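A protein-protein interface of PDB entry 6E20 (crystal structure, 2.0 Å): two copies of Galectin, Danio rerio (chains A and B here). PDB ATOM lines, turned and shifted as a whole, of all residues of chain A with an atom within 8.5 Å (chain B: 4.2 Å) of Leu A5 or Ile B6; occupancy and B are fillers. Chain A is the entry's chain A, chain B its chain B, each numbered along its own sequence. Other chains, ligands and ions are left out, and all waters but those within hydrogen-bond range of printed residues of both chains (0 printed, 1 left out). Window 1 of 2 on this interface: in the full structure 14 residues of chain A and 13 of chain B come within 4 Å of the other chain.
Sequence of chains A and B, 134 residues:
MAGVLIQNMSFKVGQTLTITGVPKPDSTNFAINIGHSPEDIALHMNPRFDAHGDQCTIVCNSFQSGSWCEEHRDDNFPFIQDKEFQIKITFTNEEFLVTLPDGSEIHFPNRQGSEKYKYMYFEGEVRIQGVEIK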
ATOM      1  N   ALA A   2      -1.752  -6.631   7.109  1.00  0.00           N
ATOM      2  CA  ALA A   2      -2.102  -5.398   7.893  1.00  0.00           C
ATOM      3  C   ALA A   2      -3.575  -5.438   8.329  1.00  0.00           C
ATOM      4  O   ALA A   2      -3.865  -4.976   9.462  1.00  0.00           O
ATOM      5  CB  ALA A   2      -1.805  -4.168   7.074  1.00  0.00           C
ATOM      6  N   GLY A   3      -4.456  -5.972   7.470  1.00  0.00           N
ATOM      7  CA  GLY A   3      -5.909  -6.113   7.706  1.00  0.00           C
ATOM      8  C   GLY A   3      -6.293  -7.517   8.154  1.00  0.00           C
ATOM      9  O   GLY A   3      -5.428  -8.242   8.660  1.00  0.00           O
ATOM     10  N   VAL A   4      -7.565  -7.887   8.026  1.00  0.00           N
ATOM     11  CA  VAL A   4      -8.105  -9.166   8.583  1.00  0.00           C
ATOM     12  C   VAL A   4      -7.827 -10.304   7.583  1.00  0.00           C
ATOM     13  O   VAL A   4      -8.308 -10.211   6.432  1.00  0.00           O
ATOM     14  CB  VAL A   4      -9.602  -9.068   8.931  1.00  0.00           C
ATOM     15  CG1 VAL A   4     -10.163 -10.419   9.372  1.00  0.00           C
ATOM     16  CG2 VAL A   4      -9.870  -8.003   9.990  1.00  0.00           C
ATOM     17  N   LEU A   5      -7.126 -11.340   8.052  1.00  0.00           N
ATOM     18  CA  LEU A   5      -6.776 -12.593   7.323  1.00  0.00           C
ATOM     19  C   LEU A   5      -7.558 -13.763   7.928  1.00  0.00           C
ATOM     20  O   LEU A   5      -7.478 -13.986   9.155  1.00  0.00           O
ATOM     21  CB  LEU A   5      -5.269 -12.818   7.443  1.00  0.00           C
ATOM     22  CG  LEU A   5      -4.719 -14.027   6.685  1.00  0.00           C
ATOM     23  CD1 LEU A   5      -5.119 -13.970   5.225  1.00  0.00           C
ATOM     24  CD2 LEU A   5      -3.205 -14.113   6.825  1.00  0.00           C
ATOM     25  N   ILE A   6      -8.348 -14.457   7.108  1.00  0.00           N
ATOM     26  CA  ILE A   6      -9.119 -15.665   7.509  1.00  0.00           C
ATOM     27  C   ILE A   6      -8.674 -16.821   6.616  1.00  0.00           C
ATOM     28  O   ILE A   6      -8.938 -16.742   5.399  1.00  0.00           O
ATOM     29  CB  ILE A   6     -10.627 -15.380   7.402  1.00  0.00           C
ATOM     30  CG1 ILE A   6     -11.022 -14.194   8.289  1.00  0.00           C
ATOM     31  CG2 ILE A   6     -11.458 -16.621   7.705  1.00  0.00           C
ATOM     32  CD1 ILE A   6     -12.506 -14.033   8.458  1.00  0.00           C
ATOM     33  N   GLN A   7      -8.032 -17.844   7.182  1.00  0.00           N
ATOM     34  CA  GLN A   7      -7.572 -19.041   6.426  1.00  0.00           C
ATOM     35  C   GLN A   7      -8.393 -20.276   6.834  1.00  0.00           C
ATOM     36  O   GLN A   7      -8.611 -20.484   8.050  1.00  0.00           O
ATOM     37  CB  GLN A   7      -6.076 -19.237   6.646  1.00  0.00           C
ATOM     38  CG  GLN A   7      -5.280 -17.965   6.371  1.00  0.00           C
ATOM     39  CD  GLN A   7      -3.816 -18.126   6.681  1.00  0.00           C
ATOM     40  OE1 GLN A   7      -3.326 -17.671   7.711  1.00  0.00           O
ATOM     41  NE2 GLN A   7      -3.110 -18.802   5.789  1.00  0.00           N
ATOM     42  N   ASN A   8      -8.845 -21.038   5.829  1.00  0.00           N
ATOM     43  CA  ASN A   8      -9.450 -22.399   5.916  1.00  0.00           C
ATOM     44  C   ASN A   8     -10.898 -22.342   6.380  1.00  0.00           C
ATOM     45  O   ASN A   8     -11.446 -23.416   6.702  1.00  0.00           O
ATOM     46  CB  ASN A   8      -8.671 -23.344   6.820  1.00  0.00           C
ATOM     47  CG  ASN A   8      -7.303 -23.659   6.265  1.00  0.00           C
ATOM     48  OD1 ASN A   8      -7.108 -23.666   5.049  1.00  0.00           O
ATOM     49  ND2 ASN A   8      -6.361 -23.917   7.156  1.00  0.00           N
ATOM     50  N   MET A   9     -11.517 -21.161   6.367  1.00  0.00           N
ATOM     51  CA  MET A   9     -12.994 -21.043   6.405  1.00  0.00           C
ATOM     52  C   MET A   9     -13.494 -21.303   4.977  1.00  0.00           C
ATOM     53  O   MET A   9     -12.909 -20.731   4.067  1.00  0.00           O
ATOM     54  CB  MET A   9     -13.395 -19.654   6.896  1.00  0.00           C
ATOM     55  CG  MET A   9     -14.637 -19.653   7.700  1.00  0.00           C
ATOM     56  SD  MET A   9     -14.926 -18.106   8.572  1.00  0.00           S
ATOM     57  CE  MET A   9     -16.704 -18.319   8.728  1.00  0.00           C
ATOM     58  N   ASN A  33     -11.156  -9.647  -0.250  1.00  0.00           N
ATOM     59  CA  ASN A  33     -10.388 -10.547  -1.139  1.00  0.00           C
ATOM     60  C   ASN A  33     -10.837 -11.982  -0.861  1.00  0.00           C
ATOM     61  O   ASN A  33     -10.858 -12.403   0.321  1.00  0.00           O
ATOM     62  CB  ASN A  33      -8.881 -10.339  -1.020  1.00  0.00           C
ATOM     63  CG  ASN A  33      -8.445  -8.923  -1.346  1.00  0.00           C
ATOM     64  OD1 ASN A  33      -8.387  -8.534  -2.508  1.00  0.00           O
ATOM     65  ND2 ASN A  33      -8.070  -8.162  -0.332  1.00  0.00           N
ATOM     66  N   HIS A  36      -7.449 -18.322  -3.178  1.00  0.00           N
ATOM     67  CA  HIS A  36      -6.715 -19.516  -2.696  1.00  0.00           C
ATOM     68  C   HIS A  36      -5.582 -19.041  -1.798  1.00  0.00           C
ATOM     69  O   HIS A  36      -5.303 -19.702  -0.800  1.00  0.00           O
ATOM     70  CB  HIS A  36      -6.173 -20.344  -3.881  1.00  0.00           C
ATOM     71  CG  HIS A  36      -7.250 -20.919  -4.735  1.00  0.00           C
ATOM     72  ND1 HIS A  36      -8.430 -21.418  -4.202  1.00  0.00           N
ATOM     73  CD2 HIS A  36      -7.350 -21.067  -6.075  1.00  0.00           C
ATOM     74  CE1 HIS A  36      -9.197 -21.865  -5.178  1.00  0.00           C
ATOM     75  NE2 HIS A  36      -8.560 -21.655  -6.330  1.00  0.00           N
ATOM     76  N   SER A  37      -4.961 -17.936  -2.198  1.00  0.00           N
ATOM     77  CA  SER A  37      -3.662 -17.439  -1.694  1.00  0.00           C
ATOM     78  C   SER A  37      -3.634 -15.924  -1.860  1.00  0.00           C
ATOM     79  O   SER A  37      -4.541 -15.365  -2.473  1.00  0.00           O
ATOM     80  CB  SER A  37      -2.523 -18.101  -2.429  1.00  0.00           C
ATOM     81  OG  SER A  37      -2.073 -17.309  -3.521  1.00  0.00           O
ATOM     82  N   PRO A  38      -2.625 -15.224  -1.295  1.00  0.00           N
ATOM     83  CA  PRO A  38      -2.375 -13.820  -1.617  1.00  0.00           C
ATOM     84  C   PRO A  38      -2.034 -13.529  -3.085  1.00  0.00           C
ATOM     85  O   PRO A  38      -2.349 -12.443  -3.529  1.00  0.00           O
ATOM     86  CB  PRO A  38      -1.152 -13.464  -0.757  1.00  0.00           C
ATOM     87  CG  PRO A  38      -1.190 -14.452   0.380  1.00  0.00           C
ATOM     88  CD  PRO A  38      -1.748 -15.717  -0.219  1.00  0.00           C
ATOM     89  N   LYS A 118     -10.786 -20.911   0.161  1.00  0.00           N
ATOM     90  CA  LYS A 118     -10.288 -21.178   1.543  1.00  0.00           C
ATOM     91  C   LYS A 118      -9.341 -20.053   2.029  1.00  0.00           C
ATOM     92  O   LYS A 118      -8.589 -20.265   3.016  1.00  0.00           O
ATOM     93  CB  LYS A 118      -9.612 -22.557   1.573  1.00  0.00           C
ATOM     94  CG  LYS A 118      -8.083 -22.602   1.511  1.00  0.00           C
ATOM     95  CD  LYS A 118      -7.392 -21.747   0.446  1.00  0.00           C
ATOM     96  CE  LYS A 118      -7.313 -22.413  -0.908  1.00  0.00           C
ATOM     97  NZ  LYS A 118      -8.622 -22.381  -1.605  1.00  0.00           N
ATOM     98  N   TYR A 119      -9.328 -18.901   1.358  1.00  0.00           N
ATOM     99  CA  TYR A 119      -8.496 -17.741   1.762  1.00  0.00           C
ATOM    100  C   TYR A 119      -9.342 -16.474   1.638  1.00  0.00           C
ATOM    101  O   TYR A 119      -9.870 -16.218   0.527  1.00  0.00           O
ATOM    102  CB  TYR A 119      -7.221 -17.691   0.924  1.00  0.00           C
ATOM    103  CG  TYR A 119      -6.453 -16.401   1.023  1.00  0.00           C
ATOM    104  CD1 TYR A 119      -6.856 -15.276   0.317  1.00  0.00           C
ATOM    105  CD2 TYR A 119      -5.307 -16.305   1.798  1.00  0.00           C
ATOM    106  CE1 TYR A 119      -6.146 -14.086   0.392  1.00  0.00           C
ATOM    107  CE2 TYR A 119      -4.592 -15.122   1.892  1.00  0.00           C
ATOM    108  CZ  TYR A 119      -5.014 -14.005   1.189  1.00  0.00           C
ATOM    109  OH  TYR A 119      -4.316 -12.832   1.256  1.00  0.00           O
ATOM    110  N   MET A 120      -9.460 -15.707   2.726  1.00  0.00           N
ATOM    111  CA  MET A 120     -10.151 -14.387   2.718  1.00  0.00           C
ATOM    112  C   MET A 120      -9.285 -13.337   3.413  1.00  0.00           C
ATOM    113  O   MET A 120      -8.775 -13.621   4.532  1.00  0.00           O
ATOM    114  CB  MET A 120     -11.528 -14.442   3.381  1.00  0.00           C
ATOM    115  CG  MET A 120     -12.447 -15.497   2.776  1.00  0.00           C
ATOM    116  SD  MET A 120     -14.099 -15.429   3.471  1.00  0.00           S
ATOM    117  CE  MET A 120     -14.395 -17.149   3.865  1.00  0.00           C
ATOM    118  N   TYR A 121      -9.098 -12.190   2.750  1.00  0.00           N
ATOM    119  CA  TYR A 121      -8.258 -11.063   3.235  1.00  0.00           C
ATOM    120  C   TYR A 121      -9.015  -9.744   3.049  1.00  0.00           C
ATOM    121  O   TYR A 121      -9.379  -9.398   1.911  1.00  0.00           O
ATOM    122  CB  TYR A 121      -6.898 -10.995   2.532  1.00  0.00           C
ATOM    123  CG  TYR A 121      -5.992  -9.925   3.086  1.00  0.00           C
ATOM    124  CD1 TYR A 121      -6.005  -9.632   4.436  1.00  0.00           C
ATOM    125  CD2 TYR A 121      -5.139  -9.181   2.289  1.00  0.00           C
ATOM    126  CE1 TYR A 121      -5.197  -8.652   4.983  1.00  0.00           C
ATOM    127  CE2 TYR A 121      -4.315  -8.199   2.823  1.00  0.00           C
ATOM    128  CZ  TYR A 121      -4.344  -7.926   4.181  1.00  0.00           C
ATOM    129  OH  TYR A 121      -3.560  -6.964   4.781  1.00  0.00           O
ATOM    130  N   PHE A 122      -9.239  -9.034   4.152  1.00  0.00           N
ATOM    131  CA  PHE A 122      -9.930  -7.734   4.186  1.00  0.00           C
ATOM    132  C   PHE A 122      -8.862  -6.669   4.407  1.00  0.00           C
ATOM    133  O   PHE A 122      -8.006  -6.811   5.320  1.00  0.00           O
ATOM    134  CB  PHE A 122     -11.050  -7.757   5.225  1.00  0.00           C
ATOM    135  CG  PHE A 122     -12.021  -8.903   5.102  1.00  0.00           C
ATOM    136  CD1 PHE A 122     -11.764 -10.133   5.697  1.00  0.00           C
ATOM    137  CD2 PHE A 122     -13.205  -8.756   4.403  1.00  0.00           C
ATOM    138  CE1 PHE A 122     -12.661 -11.184   5.585  1.00  0.00           C
ATOM    139  CE2 PHE A 122     -14.105  -9.801   4.303  1.00  0.00           C
ATOM    140  CZ  PHE A 122     -13.827 -11.019   4.886  1.00  0.00           C
ATOM    141  N   GLU A 123      -8.865  -5.668   3.528  1.00  0.00           N
ATOM    142  CA  GLU A 123      -7.840  -4.604   3.439  1.00  0.00           C
ATOM    143  C   GLU A 123      -8.517  -3.257   3.673  1.00  0.00           C
ATOM    144  O   GLU A 123      -9.731  -3.123   3.356  1.00  0.00           O
ATOM    145  CB  GLU A 123      -7.178  -4.553   2.058  1.00  0.00           C
ATOM    146  CG  GLU A 123      -6.701  -5.891   1.529  1.00  0.00           C
ATOM    147  CD  GLU A 123      -5.851  -5.793   0.267  1.00  0.00           C
ATOM    148  OE1 GLU A 123      -6.432  -5.614  -0.852  1.00  0.00           O
ATOM    149  OE2 GLU A 123      -4.602  -5.859   0.406  1.00  0.00           O
ATOM    150  N   ILE A 128     -14.079  -5.099  10.214  1.00  0.00           N
ATOM    151  CA  ILE A 128     -14.865  -6.327   9.901  1.00  0.00           C
ATOM    152  C   ILE A 128     -15.478  -6.845  11.204  1.00  0.00           C
ATOM    153  O   ILE A 128     -14.705  -7.232  12.111  1.00  0.00           O
ATOM    154  CB  ILE A 128     -13.988  -7.380   9.203  1.00  0.00           C
ATOM    155  CG1 ILE A 128     -13.428  -6.849   7.880  1.00  0.00           C
ATOM    156  CG2 ILE A 128     -14.763  -8.678   9.038  1.00  0.00           C
ATOM    157  CD1 ILE A 128     -14.455  -6.206   6.986  1.00  0.00           C
ATOM    158  N   VAL A 131     -18.350 -12.374   9.659  1.00  0.00           N
ATOM    159  CA  VAL A 131     -18.020 -13.284   8.526  1.00  0.00           C
ATOM    160  C   VAL A 131     -18.769 -14.607   8.717  1.00  0.00           C
ATOM    161  O   VAL A 131     -18.408 -15.336   9.642  1.00  0.00           O
ATOM    162  CB  VAL A 131     -16.505 -13.492   8.402  1.00  0.00           C
ATOM    163  CG1 VAL A 131     -16.158 -14.412   7.243  1.00  0.00           C
ATOM    164  CG2 VAL A 131     -15.774 -12.159   8.285  1.00  0.00           C
ATOM    165  N   LEU B   5      -7.760 -20.060  10.999  1.00  0.00           N
ATOM    166  CA  LEU B   5      -6.949 -18.997  11.645  1.00  0.00           C
ATOM    167  C   LEU B   5      -7.553 -17.646  11.277  1.00  0.00           C
ATOM    168  O   LEU B   5      -7.799 -17.399  10.092  1.00  0.00           O
ATOM    169  CB  LEU B   5      -5.495 -19.103  11.193  1.00  0.00           C
ATOM    170  CG  LEU B   5      -4.539 -18.161  11.925  1.00  0.00           C
ATOM    171  CD1 LEU B   5      -4.530 -18.496  13.409  1.00  0.00           C
ATOM    172  CD2 LEU B   5      -3.125 -18.229  11.345  1.00  0.00           C
ATOM    173  N   ILE B   6      -7.859 -16.826  12.273  1.00  0.00           N
ATOM    174  CA  ILE B   6      -8.375 -15.451  12.049  1.00  0.00           C
ATOM    175  C   ILE B   6      -7.420 -14.483  12.738  1.00  0.00           C
ATOM    176  O   ILE B   6      -7.311 -14.580  13.981  1.00  0.00           O
ATOM    177  CB  ILE B   6      -9.817 -15.322  12.556  1.00  0.00           C
ATOM    178  CG1 ILE B   6     -10.685 -16.377  11.861  1.00  0.00           C
ATOM    179  CG2 ILE B   6     -10.327 -13.894  12.397  1.00  0.00           C
ATOM    180  CD1 ILE B   6     -12.132 -16.294  12.141  1.00  0.00           C
ATOM    181  N   GLN B   7      -6.785 -13.599  11.961  1.00  0.00           N
ATOM    182  CA  GLN B   7      -5.841 -12.584  12.492  1.00  0.00           C
ATOM    183  C   GLN B   7      -6.394 -11.180  12.269  1.00  0.00           C
ATOM    184  O   GLN B   7      -6.799 -10.862  11.128  1.00  0.00           O
ATOM    185  CB  GLN B   7      -4.469 -12.749  11.860  1.00  0.00           C
ATOM    186  CG  GLN B   7      -3.801 -14.042  12.280  1.00  0.00           C
ATOM    187  CD  GLN B   7      -2.584 -14.314  11.435  1.00  0.00           C
ATOM    188  OE1 GLN B   7      -2.694 -14.599  10.241  1.00  0.00           O
ATOM    189  NE2 GLN B   7      -1.421 -14.214  12.061  1.00  0.00           N
ATOM    190  N   MET B   9      -8.918  -9.515  13.524  1.00  0.00           N
ATOM    191  CA  MET B   9     -10.350  -9.238  13.816  1.00  0.00           C
ATOM    192  C   MET B   9     -10.483  -8.946  15.320  1.00  0.00           C
ATOM    193  O   MET B   9     -10.678  -9.864  16.086  1.00  0.00           O
ATOM    194  CB  MET B   9     -11.213 -10.432  13.407  1.00  0.00           C
ATOM    195  CG  MET B   9     -12.677 -10.097  13.268  1.00  0.00           C
ATOM    196  SD  MET B   9     -13.656 -11.501  12.692  1.00  0.00           S
ATOM    197  CE  MET B   9     -15.298 -10.797  12.819  1.00  0.00           C
ATOM    198  N   LYS B 118      -6.297 -10.185  19.149  1.00  0.00           N
ATOM    199  CA  LYS B 118      -6.322 -10.092  17.664  1.00  0.00           C
ATOM    200  C   LYS B 118      -5.906 -11.437  17.035  1.00  0.00           C
ATOM    201  O   LYS B 118      -5.739 -11.489  15.782  1.00  0.00           O
ATOM    202  CB  LYS B 118      -5.453  -8.907  17.240  1.00  0.00           C
ATOM    203  CG  LYS B 118      -6.034  -7.562  17.666  1.00  0.00           C
ATOM    204  CD  LYS B 118      -5.088  -6.380  17.549  1.00  0.00           C
ATOM    205  CE  LYS B 118      -4.310  -6.344  16.256  1.00  0.00           C
ATOM    206  NZ  LYS B 118      -3.560  -5.071  16.122  1.00  0.00           N
ATOM    207  N   TYR B 119      -5.830 -12.495  17.844  1.00  0.00           N
ATOM    208  CA  TYR B 119      -5.522 -13.873  17.388  1.00  0.00           C
ATOM    209  C   TYR B 119      -6.676 -14.819  17.754  1.00  0.00           C
ATOM    210  O   TYR B 119      -7.034 -14.934  18.933  1.00  0.00           O
ATOM    211  CB  TYR B 119      -4.165 -14.291  17.961  1.00  0.00           C
ATOM    212  CG  TYR B 119      -3.783 -15.699  17.613  1.00  0.00           C
ATOM    213  CD1 TYR B 119      -3.109 -16.011  16.447  1.00  0.00           C
ATOM    214  CD2 TYR B 119      -4.161 -16.730  18.441  1.00  0.00           C
ATOM    215  CE1 TYR B 119      -2.791 -17.323  16.134  1.00  0.00           C
ATOM    216  CE2 TYR B 119      -3.844 -18.041  18.148  1.00  0.00           C
ATOM    217  CZ  TYR B 119      -3.159 -18.340  16.990  1.00  0.00           C
ATOM    218  OH  TYR B 119      -2.873 -19.654  16.760  1.00  0.00           O
ATOM    219  N   MET B 120      -7.290 -15.470  16.763  1.00  0.00           N
ATOM    220  CA  MET B 120      -8.317 -16.526  17.002  1.00  0.00           C
ATOM    221  C   MET B 120      -7.962 -17.751  16.152  1.00  0.00           C
ATOM    222  O   MET B 120      -7.674 -17.623  14.950  1.00  0.00           O
ATOM    223  CB  MET B 120      -9.744 -16.074  16.676  1.00  0.00           C
ATOM    224  CG  MET B 120     -10.271 -15.018  17.609  1.00  0.00           C
ATOM    225  SD  MET B 120     -12.025 -14.658  17.312  1.00  0.00           S
ATOM    226  CE  MET B 120     -11.936 -13.560  15.900  1.00  0.00           C
ATOM    227  N   PHE B 122      -9.241 -21.864  15.592  1.00  0.00           N
ATOM    228  CA  PHE B 122     -10.200 -22.970  15.795  1.00  0.00           C
ATOM    229  C   PHE B 122      -9.530 -24.255  15.318  1.00  0.00           C
ATOM    230  O   PHE B 122      -9.136 -24.316  14.141  1.00  0.00           O
ATOM    231  CB  PHE B 122     -11.501 -22.675  15.052  1.00  0.00           C
ATOM    232  CG  PHE B 122     -12.063 -21.305  15.323  1.00  0.00           C
ATOM    233  CD1 PHE B 122     -11.627 -20.203  14.612  1.00  0.00           C
ATOM    234  CD2 PHE B 122     -12.968 -21.106  16.343  1.00  0.00           C
ATOM    235  CE1 PHE B 122     -12.152 -18.945  14.871  1.00  0.00           C
ATOM    236  CE2 PHE B 122     -13.485 -19.848  16.610  1.00  0.00           C
ATOM    237  CZ  PHE B 122     -13.075 -18.767  15.870  1.00  0.00           C
ATOM    238  N   VAL B 131     -18.158 -16.204  12.379  1.00  0.00           N
ATOM    239  CA  VAL B 131     -17.482 -15.407  13.434  1.00  0.00           C
ATOM    240  C   VAL B 131     -18.024 -13.986  13.322  1.00  0.00           C
ATOM    241  O   VAL B 131     -17.833 -13.361  12.248  1.00  0.00           O
ATOM    242  CB  VAL B 131     -15.951 -15.444  13.328  1.00  0.00           C
ATOM    243  CG1 VAL B 131     -15.296 -14.778  14.535  1.00  0.00           C
ATOM    244  CG2 VAL B 131     -15.467 -16.873  13.198  1.00  0.00           C
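O of Leu A5 is in hydrogen-bond range of N of Gln B7 (2.9 Å). The backbone NH (N) of Gln A7 lies within hydrogen-bond range of the backbone carbonyl oxygen (O) of Leu B5, at 3.0 Å. N of Val A131 lies within hydrogen-bond range of O of Val B131 (2.8 Å).
The backbone NH (N) of Gly A3 is in hydrogen-bond range of the side-chain hydroxyl (OH) of Tyr A121 (3.0 Å). O of Val A4 is in hydrogen-bond range of N of Phe A122, 2.7 Å away. N of Ile A6 is in hydrogen-bond range of O of Met A120 (2.7 Å). The backbone NH (N) of Ile B6 lies within hydrogen-bond range of the backbone carbonyl oxygen (O) of Met B120 (2.8 Å).
O of Gly A3 touches O of Gln B7, 3.9 Å away. Val A4 touches Gln B7 (CA to O, 3.3 Å). Val A4 touches Met B9 (CG2 to N, 3.96 Å). Leu B5 touches Leu A5. Leu A5 touches Ile B6 (O to CA, 3.4 Å). Leu B5 touches Ile A6 (O to CA, 3.4 Å). Met B9 touches Ile A128 (CE to O, 3.7 Å).
Ala A2 touches none of the printed residues of chain B. Leu A5 touches three residues of chain B. Printed residues of chain B within 4 Å of Gln A7: Leu B5. Of the printed residues of chain B, Ile A128 touches Met B9 (3.7 Å). Printed residues of chain B within 4 Å of Val A131: Val B131 (2.8 Å). Of the printed residues of chain A, Gln B7 touches Gly A3 (3.9 Å), Val A4 (3.3 Å) and Leu A5 (2.9 Å). Printed residues of chain A within 4 Å of Met B9: Val A4 (3.96 Å) and Ile A128 (3.7 Å). The nearest printed residue of chain B that does not touch Leu A5 is Met B9 (6.0 Å). The nearest residue of chain A that does not touch Ile B6 is Ile A6 (4.2 Å).
Of the 9 printed residues of chain B, 5 touch a printed residue of chain A. Printed residues of chain A that touch a printed residue of chain B: Gly A3, Val A4, Leu A5, Ile A6, Gln A7, Ile A128 and Val A131. Among the printed residues, 10 pairs touch across the chains. Among the printed residues, no Asp or Glu carboxylate lies within 4 Å of a Lys or Arg side-chain nitrogen of the other chain.
Leu B5 touches its own counterpart, Leu A5. Leu A5 touches Ile B6, and with the chains exchanged Ile A6 touches Leu B5. Leu A5 touches Gln B7, and with the chains exchanged Gln A7 touches Leu B5. Val B131 touches its own counterpart, Val A131. Positions printed for both chains: 5, 6, 7, 9, 118, 119, 120, 122 and 131.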
